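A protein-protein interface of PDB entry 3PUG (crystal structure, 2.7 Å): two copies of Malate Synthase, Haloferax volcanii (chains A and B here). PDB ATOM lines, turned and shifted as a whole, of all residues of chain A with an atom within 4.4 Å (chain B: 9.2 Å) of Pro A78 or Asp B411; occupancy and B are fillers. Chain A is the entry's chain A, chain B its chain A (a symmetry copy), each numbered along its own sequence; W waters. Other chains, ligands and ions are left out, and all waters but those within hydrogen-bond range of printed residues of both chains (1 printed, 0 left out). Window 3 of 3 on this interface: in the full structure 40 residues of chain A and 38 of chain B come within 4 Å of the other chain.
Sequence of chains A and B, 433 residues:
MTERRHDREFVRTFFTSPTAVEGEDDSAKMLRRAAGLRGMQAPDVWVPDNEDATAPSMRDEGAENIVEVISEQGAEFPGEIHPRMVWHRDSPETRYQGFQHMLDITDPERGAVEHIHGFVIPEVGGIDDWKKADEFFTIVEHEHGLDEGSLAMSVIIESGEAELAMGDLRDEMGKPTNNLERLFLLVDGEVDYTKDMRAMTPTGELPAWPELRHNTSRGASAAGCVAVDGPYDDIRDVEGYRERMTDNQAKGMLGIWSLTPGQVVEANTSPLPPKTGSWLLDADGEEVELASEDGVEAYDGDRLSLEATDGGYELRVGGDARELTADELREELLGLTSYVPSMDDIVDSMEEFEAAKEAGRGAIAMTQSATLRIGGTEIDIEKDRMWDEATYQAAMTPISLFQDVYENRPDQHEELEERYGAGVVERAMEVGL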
ATOM      1  N   LEU A  37     -18.962   7.402 -12.941  1.00  0.00           N
ATOM      2  CA  LEU A  37     -17.543   7.426 -12.625  1.00  0.00           C
ATOM      3  C   LEU A  37     -17.345   6.435 -11.505  1.00  0.00           C
ATOM      4  O   LEU A  37     -18.200   6.351 -10.628  1.00  0.00           O
ATOM      5  CB  LEU A  37     -17.199   8.809 -12.110  1.00  0.00           C
ATOM      6  CG  LEU A  37     -17.015   9.847 -13.219  1.00  0.00           C
ATOM      7  CD1 LEU A  37     -16.541  11.136 -12.526  1.00  0.00           C
ATOM      8  CD2 LEU A  37     -16.027   9.482 -14.325  1.00  0.00           C
ATOM      9  N   ARG A  38     -16.247   5.687 -11.537  1.00  0.00           N
ATOM     10  CA  ARG A  38     -15.996   4.663 -10.520  1.00  0.00           C
ATOM     11  C   ARG A  38     -14.510   4.752 -10.180  1.00  0.00           C
ATOM     12  O   ARG A  38     -13.759   5.449 -10.873  1.00  0.00           O
ATOM     13  CB  ARG A  38     -16.428   3.267 -11.014  1.00  0.00           C
ATOM     14  CG  ARG A  38     -17.923   3.215 -11.446  1.00  0.00           C
ATOM     15  CD  ARG A  38     -18.833   3.228 -10.208  1.00  0.00           C
ATOM     16  NE  ARG A  38     -20.263   3.054 -10.430  1.00  0.00           N
ATOM     17  CZ  ARG A  38     -21.087   3.977 -10.918  1.00  0.00           C
ATOM     18  NH1 ARG A  38     -20.667   5.193 -11.278  1.00  0.00           N
ATOM     19  NH2 ARG A  38     -22.372   3.676 -11.060  1.00  0.00           N
ATOM     20  N   GLY A  39     -14.082   4.108  -9.101  1.00  0.00           N
ATOM     21  CA  GLY A  39     -12.678   4.135  -8.723  1.00  0.00           C
ATOM     22  C   GLY A  39     -12.092   5.519  -8.495  1.00  0.00           C
ATOM     23  O   GLY A  39     -12.781   6.455  -8.061  1.00  0.00           O
ATOM     24  N   ALA A  42     -13.745   8.742  -9.391  1.00  0.00           N
ATOM     25  CA  ALA A  42     -14.938   9.198  -8.635  1.00  0.00           C
ATOM     26  C   ALA A  42     -14.646  10.077  -7.391  1.00  0.00           C
ATOM     27  O   ALA A  42     -13.802   9.764  -6.546  1.00  0.00           O
ATOM     28  CB  ALA A  42     -15.838   8.038  -8.280  1.00  0.00           C
ATOM     29  N   GLU A  76     -26.039   3.640  -7.629  1.00  0.00           N
ATOM     30  CA  GLU A  76     -24.798   2.928  -7.942  1.00  0.00           C
ATOM     31  C   GLU A  76     -23.635   3.858  -7.656  1.00  0.00           C
ATOM     32  O   GLU A  76     -22.499   3.394  -7.600  1.00  0.00           O
ATOM     33  CB  GLU A  76     -24.748   2.488  -9.440  1.00  0.00           C
ATOM     34  CG  GLU A  76     -26.040   1.820  -9.975  1.00  0.00           C
ATOM     35  CD  GLU A  76     -26.277   0.505  -9.244  1.00  0.00           C
ATOM     36  OE1 GLU A  76     -25.413   0.148  -8.409  1.00  0.00           O
ATOM     37  OE2 GLU A  76     -27.304  -0.169  -9.465  1.00  0.00           O
ATOM     38  N   PHE A  77     -23.911   5.156  -7.529  1.00  0.00           N
ATOM     39  CA  PHE A  77     -22.824   6.134  -7.411  1.00  0.00           C
ATOM     40  C   PHE A  77     -22.063   5.859  -6.123  1.00  0.00           C
ATOM     41  O   PHE A  77     -22.667   5.761  -5.058  1.00  0.00           O
ATOM     42  CB  PHE A  77     -23.276   7.589  -7.559  1.00  0.00           C
ATOM     43  CG  PHE A  77     -22.149   8.556  -7.442  1.00  0.00           C
ATOM     44  CD1 PHE A  77     -21.252   8.720  -8.472  1.00  0.00           C
ATOM     45  CD2 PHE A  77     -21.939   9.268  -6.262  1.00  0.00           C
ATOM     46  CE1 PHE A  77     -20.174   9.603  -8.342  1.00  0.00           C
ATOM     47  CE2 PHE A  77     -20.870  10.148  -6.124  1.00  0.00           C
ATOM     48  CZ  PHE A  77     -19.980  10.316  -7.172  1.00  0.00           C
ATOM     49  N   PRO A  78     -20.748   5.647  -6.253  1.00  0.00           N
ATOM     50  CA  PRO A  78     -20.006   5.102  -5.125  1.00  0.00           C
ATOM     51  C   PRO A  78     -19.686   6.128  -4.018  1.00  0.00           C
ATOM     52  O   PRO A  78     -19.543   5.731  -2.859  1.00  0.00           O
ATOM     53  CB  PRO A  78     -18.731   4.559  -5.774  1.00  0.00           C
ATOM     54  CG  PRO A  78     -18.533   5.360  -6.999  1.00  0.00           C
ATOM     55  CD  PRO A  78     -19.905   5.806  -7.458  1.00  0.00           C
ATOM     56  N   GLY A  79     -19.567   7.418  -4.330  1.00  0.00           N
ATOM     57  CA  GLY A  79     -19.331   8.398  -3.284  1.00  0.00           C
ATOM     58  C   GLY A  79     -20.639   8.909  -2.695  1.00  0.00           C
ATOM     59  O   GLY A  79     -21.744   8.402  -2.982  1.00  0.00           O
ATOM     60  N   VAL B 405     -10.827   6.112   3.696  1.00  0.00           N
ATOM     61  CA  VAL B 405     -11.026   5.927   2.268  1.00  0.00           C
ATOM     62  C   VAL B 405     -11.342   4.460   1.990  1.00  0.00           C
ATOM     63  O   VAL B 405     -12.339   4.119   1.348  1.00  0.00           O
ATOM     64  CB  VAL B 405      -9.805   6.446   1.467  1.00  0.00           C
ATOM     65  CG1 VAL B 405      -9.872   6.049   0.007  1.00  0.00           C
ATOM     66  CG2 VAL B 405      -9.673   7.967   1.582  1.00  0.00           C
ATOM     67  N   TYR B 406     -10.517   3.567   2.518  1.00  0.00           N
ATOM     68  CA  TYR B 406     -10.732   2.144   2.327  1.00  0.00           C
ATOM     69  C   TYR B 406     -12.096   1.669   2.820  1.00  0.00           C
ATOM     70  O   TYR B 406     -12.717   0.816   2.201  1.00  0.00           O
ATOM     71  CB  TYR B 406      -9.629   1.320   3.002  1.00  0.00           C
ATOM     72  CG  TYR B 406      -9.619  -0.130   2.514  1.00  0.00           C
ATOM     73  CD1 TYR B 406      -8.931  -0.491   1.339  1.00  0.00           C
ATOM     74  CD2 TYR B 406     -10.333  -1.134   3.194  1.00  0.00           C
ATOM     75  CE1 TYR B 406      -8.927  -1.790   0.875  1.00  0.00           C
ATOM     76  CE2 TYR B 406     -10.343  -2.450   2.726  1.00  0.00           C
ATOM     77  CZ  TYR B 406      -9.634  -2.754   1.575  1.00  0.00           C
ATOM     78  OH  TYR B 406      -9.622  -4.044   1.116  1.00  0.00           O
ATOM     79  N   GLU B 407     -12.548   2.171   3.959  1.00  0.00           N
ATOM     80  CA  GLU B 407     -13.788   1.737   4.571  1.00  0.00           C
ATOM     81  C   GLU B 407     -14.995   2.118   3.690  1.00  0.00           C
ATOM     82  O   GLU B 407     -16.004   1.414   3.661  1.00  0.00           O
ATOM     83  CB  GLU B 407     -13.877   2.467   5.907  1.00  0.00           C
ATOM     84  CG  GLU B 407     -13.997   1.609   7.152  1.00  0.00           C
ATOM     85  CD  GLU B 407     -12.985   2.048   8.204  1.00  0.00           C
ATOM     86  OE1 GLU B 407     -12.231   2.989   7.878  1.00  0.00           O
ATOM     87  OE2 GLU B 407     -12.917   1.461   9.314  1.00  0.00           O
ATOM     88  N   ASN B 408     -14.882   3.226   2.950  1.00  0.00           N
ATOM     89  CA  ASN B 408     -16.026   3.887   2.305  1.00  0.00           C
ATOM     90  C   ASN B 408     -15.930   3.900   0.793  1.00  0.00           C
ATOM     91  O   ASN B 408     -16.841   4.344   0.110  1.00  0.00           O
ATOM     92  CB  ASN B 408     -16.159   5.327   2.810  1.00  0.00           C
ATOM     93  CG  ASN B 408     -16.537   5.401   4.282  1.00  0.00           C
ATOM     94  OD1 ASN B 408     -17.703   5.237   4.631  1.00  0.00           O
ATOM     95  ND2 ASN B 408     -15.566   5.666   5.148  1.00  0.00           N
ATOM     96  N   ARG B 409     -14.821   3.425   0.242  1.00  0.00           N
ATOM     97  CA  ARG B 409     -14.735   3.393  -1.205  1.00  0.00           C
ATOM     98  C   ARG B 409     -14.414   2.015  -1.825  1.00  0.00           C
ATOM     99  O   ARG B 409     -13.356   1.843  -2.424  1.00  0.00           O
ATOM    100  CB  ARG B 409     -13.776   4.496  -1.648  1.00  0.00           C
ATOM    101  CG  ARG B 409     -14.318   5.885  -1.418  1.00  0.00           C
ATOM    102  CD  ARG B 409     -15.568   6.181  -2.231  1.00  0.00           C
ATOM    103  NE  ARG B 409     -15.342   6.183  -3.677  1.00  0.00           N
ATOM    104  CZ  ARG B 409     -14.806   7.197  -4.341  1.00  0.00           C
ATOM    105  NH1 ARG B 409     -14.453   8.260  -3.666  1.00  0.00           N
ATOM    106  NH2 ARG B 409     -14.675   7.230  -5.655  1.00  0.00           N
ATOM    107  N   PRO B 410     -15.300   1.005  -1.676  1.00  0.00           N
ATOM    108  CA  PRO B 410     -15.145  -0.263  -2.422  1.00  0.00           C
ATOM    109  C   PRO B 410     -14.697  -0.131  -3.894  1.00  0.00           C
ATOM    110  O   PRO B 410     -13.722  -0.743  -4.328  1.00  0.00           O
ATOM    111  CB  PRO B 410     -16.548  -0.879  -2.326  1.00  0.00           C
ATOM    112  CG  PRO B 410     -17.396   0.039  -1.425  1.00  0.00           C
ATOM    113  CD  PRO B 410     -16.408   0.903  -0.703  1.00  0.00           C
ATOM    114  N   ASP B 411     -15.385   0.679  -4.683  1.00  0.00           N
ATOM    115  CA  ASP B 411     -14.942   0.987  -6.034  1.00  0.00           C
ATOM    116  C   ASP B 411     -13.450   1.336  -6.242  1.00  0.00           C
ATOM    117  O   ASP B 411     -12.913   1.289  -7.354  1.00  0.00           O
ATOM    118  CB  ASP B 411     -15.857   2.079  -6.598  1.00  0.00           C
ATOM    119  CG  ASP B 411     -15.668   3.413  -5.904  1.00  0.00           C
ATOM    120  OD1 ASP B 411     -15.968   3.508  -4.701  1.00  0.00           O
ATOM    121  OD2 ASP B 411     -15.207   4.375  -6.545  1.00  0.00           O
ATOM    122  N   GLN B 412     -12.780   1.756  -5.177  1.00  0.00           N
ATOM    123  CA  GLN B 412     -11.369   2.148  -5.233  1.00  0.00           C
ATOM    124  C   GLN B 412     -10.431   1.040  -4.749  1.00  0.00           C
ATOM    125  O   GLN B 412      -9.236   1.096  -5.040  1.00  0.00           O
ATOM    126  CB  GLN B 412     -11.126   3.422  -4.423  1.00  0.00           C
ATOM    127  CG  GLN B 412     -11.944   4.577  -4.938  1.00  0.00           C
ATOM    128  CD  GLN B 412     -11.325   5.918  -4.623  1.00  0.00           C
ATOM    129  OE1 GLN B 412     -10.530   6.037  -3.693  1.00  0.00           O
ATOM    130  NE2 GLN B 412     -11.655   6.921  -5.429  1.00  0.00           N
ATOM    131  N   HIS B 413     -10.987   0.078  -4.007  1.00  0.00           N
ATOM    132  CA  HIS B 413     -10.304  -1.104  -3.477  1.00  0.00           C
ATOM    133  C   HIS B 413      -9.327  -1.768  -4.454  1.00  0.00           C
ATOM    134  O   HIS B 413      -8.234  -2.172  -4.056  1.00  0.00           O
ATOM    135  CB  HIS B 413     -11.338  -2.143  -3.057  1.00  0.00           C
ATOM    136  CG  HIS B 413     -11.907  -1.923  -1.692  1.00  0.00           C
ATOM    137  ND1 HIS B 413     -12.373  -2.958  -0.908  1.00  0.00           N
ATOM    138  CD2 HIS B 413     -12.069  -0.800  -0.959  1.00  0.00           C
ATOM    139  CE1 HIS B 413     -12.793  -2.490   0.251  1.00  0.00           C
ATOM    140  NE2 HIS B 413     -12.631  -1.182   0.236  1.00  0.00           N
ATOM    141  N   GLU B 414      -9.710  -1.882  -5.726  1.00  0.00           N
ATOM    142  CA  GLU B 414      -8.871  -2.539  -6.726  1.00  0.00           C
ATOM    143  C   GLU B 414      -7.663  -1.671  -7.087  1.00  0.00           C
ATOM    144  O   GLU B 414      -6.536  -2.069  -6.807  1.00  0.00           O
ATOM    145  CB  GLU B 414      -9.742  -2.915  -7.927  1.00  0.00           C
ATOM    146  CG  GLU B 414      -9.190  -3.872  -8.988  1.00  0.00           C
ATOM    147  CD  GLU B 414      -9.929  -3.690 -10.325  1.00  0.00           C
ATOM    148  OE1 GLU B 414     -11.160  -3.403 -10.335  1.00  0.00           O
ATOM    149  OE2 GLU B 414      -9.261  -3.796 -11.381  1.00  0.00           O
ATOM    150  N   GLU B 415      -7.873  -0.477  -7.647  1.00  0.00           N
ATOM    151  CA  GLU B 415      -6.779   0.478  -7.887  1.00  0.00           C
ATOM    152  C   GLU B 415      -5.892   0.809  -6.671  1.00  0.00           C
ATOM    153  O   GLU B 415      -4.741   1.230  -6.824  1.00  0.00           O
ATOM    154  CB  GLU B 415      -7.286   1.793  -8.483  1.00  0.00           C
ATOM    155  CG  GLU B 415      -8.483   1.690  -9.394  1.00  0.00           C
ATOM    156  CD  GLU B 415      -8.691   2.975 -10.172  1.00  0.00           C
ATOM    157  OE1 GLU B 415      -7.685   3.571 -10.637  1.00  0.00           O
ATOM    158  OE2 GLU B 415      -9.867   3.390 -10.307  1.00  0.00           O
ATOM    159  N   LEU B 416      -6.423   0.660  -5.463  1.00  0.00           N
ATOM    160  CA  LEU B 416      -5.630   0.977  -4.288  1.00  0.00           C
ATOM    161  C   LEU B 416      -4.620  -0.138  -4.142  1.00  0.00           C
ATOM    162  O   LEU B 416      -3.435   0.123  -3.925  1.00  0.00           O
ATOM    163  CB  LEU B 416      -6.478   1.166  -3.017  1.00  0.00           C
ATOM    164  CG  LEU B 416      -7.070   2.551  -2.696  1.00  0.00           C
ATOM    165  CD1 LEU B 416      -8.069   2.480  -1.576  1.00  0.00           C
ATOM    166  CD2 LEU B 416      -6.014   3.617  -2.397  1.00  0.00           C
ATOM    167  N   GLU B 417      -5.098  -1.373  -4.302  1.00  0.00           N
ATOM    168  CA  GLU B 417      -4.229  -2.552  -4.240  1.00  0.00           C
ATOM    169  C   GLU B 417      -3.224  -2.615  -5.381  1.00  0.00           C
ATOM    170  O   GLU B 417      -2.070  -2.929  -5.163  1.00  0.00           O
ATOM    171  CB  GLU B 417      -5.033  -3.841  -4.064  1.00  0.00           C
ATOM    172  CG  GLU B 417      -5.277  -4.116  -2.590  1.00  0.00           C
ATOM    173  CD  GLU B 417      -6.328  -5.167  -2.321  1.00  0.00           C
ATOM    174  OE1 GLU B 417      -7.463  -5.037  -2.839  1.00  0.00           O
ATOM    175  OE2 GLU B 417      -6.010  -6.107  -1.557  1.00  0.00           O
HETATM  176  O   HOH W   1     -19.472   4.312  -0.540  1.00  0.00           O
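O of Gly A39 lies within hydrogen-bond range of NH2 of Arg B409, 3.2 Å away. The guanidinium group (NH2) of Arg B409 is in hydrogen-bond range of the backbone carbonyl oxygen (O) of Ala A42 (2.8 Å). NE2 of Gln B412 sits at hydrogen-bond distance from O of Gly A39 (2.9 Å). The backbone NH (N) of Gly A39 lies within hydrogen-bond range of the side-chain carboxylate (OD2) of Asp B411 (2.8 Å).
The guanidinium group (NH2) of Arg B409 lies close to the side-chain amide nitrogen (NE2) of Gln B412, 3.0 Å away. OD1 of Asp B411 lies within salt-bridge range of NE of Arg B409, at 2.9 Å. NH2 of Arg A38 sits close to O of Glu A76 (3.5 Å).
Among the printed residues, pairs that only touch across the chains: Arg A38 with Asp B411, Gly A39 with Glu B415, Ala A42 with Gln B412 and Pro A78 with Asp B411.
Gly A39 touches just these residues of chain B: Arg B409, Asp B411, Gln B412 and Glu B415. No residue of chain B comes within 4 Å of Phe A77. Printed residues of chain A within 4 Å of Arg B409: Gly A39 and Ala A42. Of chain A, only Arg A38, Gly A39 and Pro A78 come within 4 Å of Asp B411. Printed residues of chain A within 4 Å of Glu B415: Gly A39 (3.3 Å). The nearest residue of chain A that does not touch Asp B411 is Ala A42 (4.1 Å). The nearest printed residue of chain A that does not touch Gln B412 is Arg A38 (5.8 Å).
Printed residues of chain B that touch a printed residue of chain A: Arg B409, Asp B411, Gln B412 and Glu B415.
No position is printed for both chains.
Water W1 lies within hydrogen-bond range of the backbone carbonyl oxygen (O) of Asn B408 and the backbone carbonyl oxygen (O) of Pro A78.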
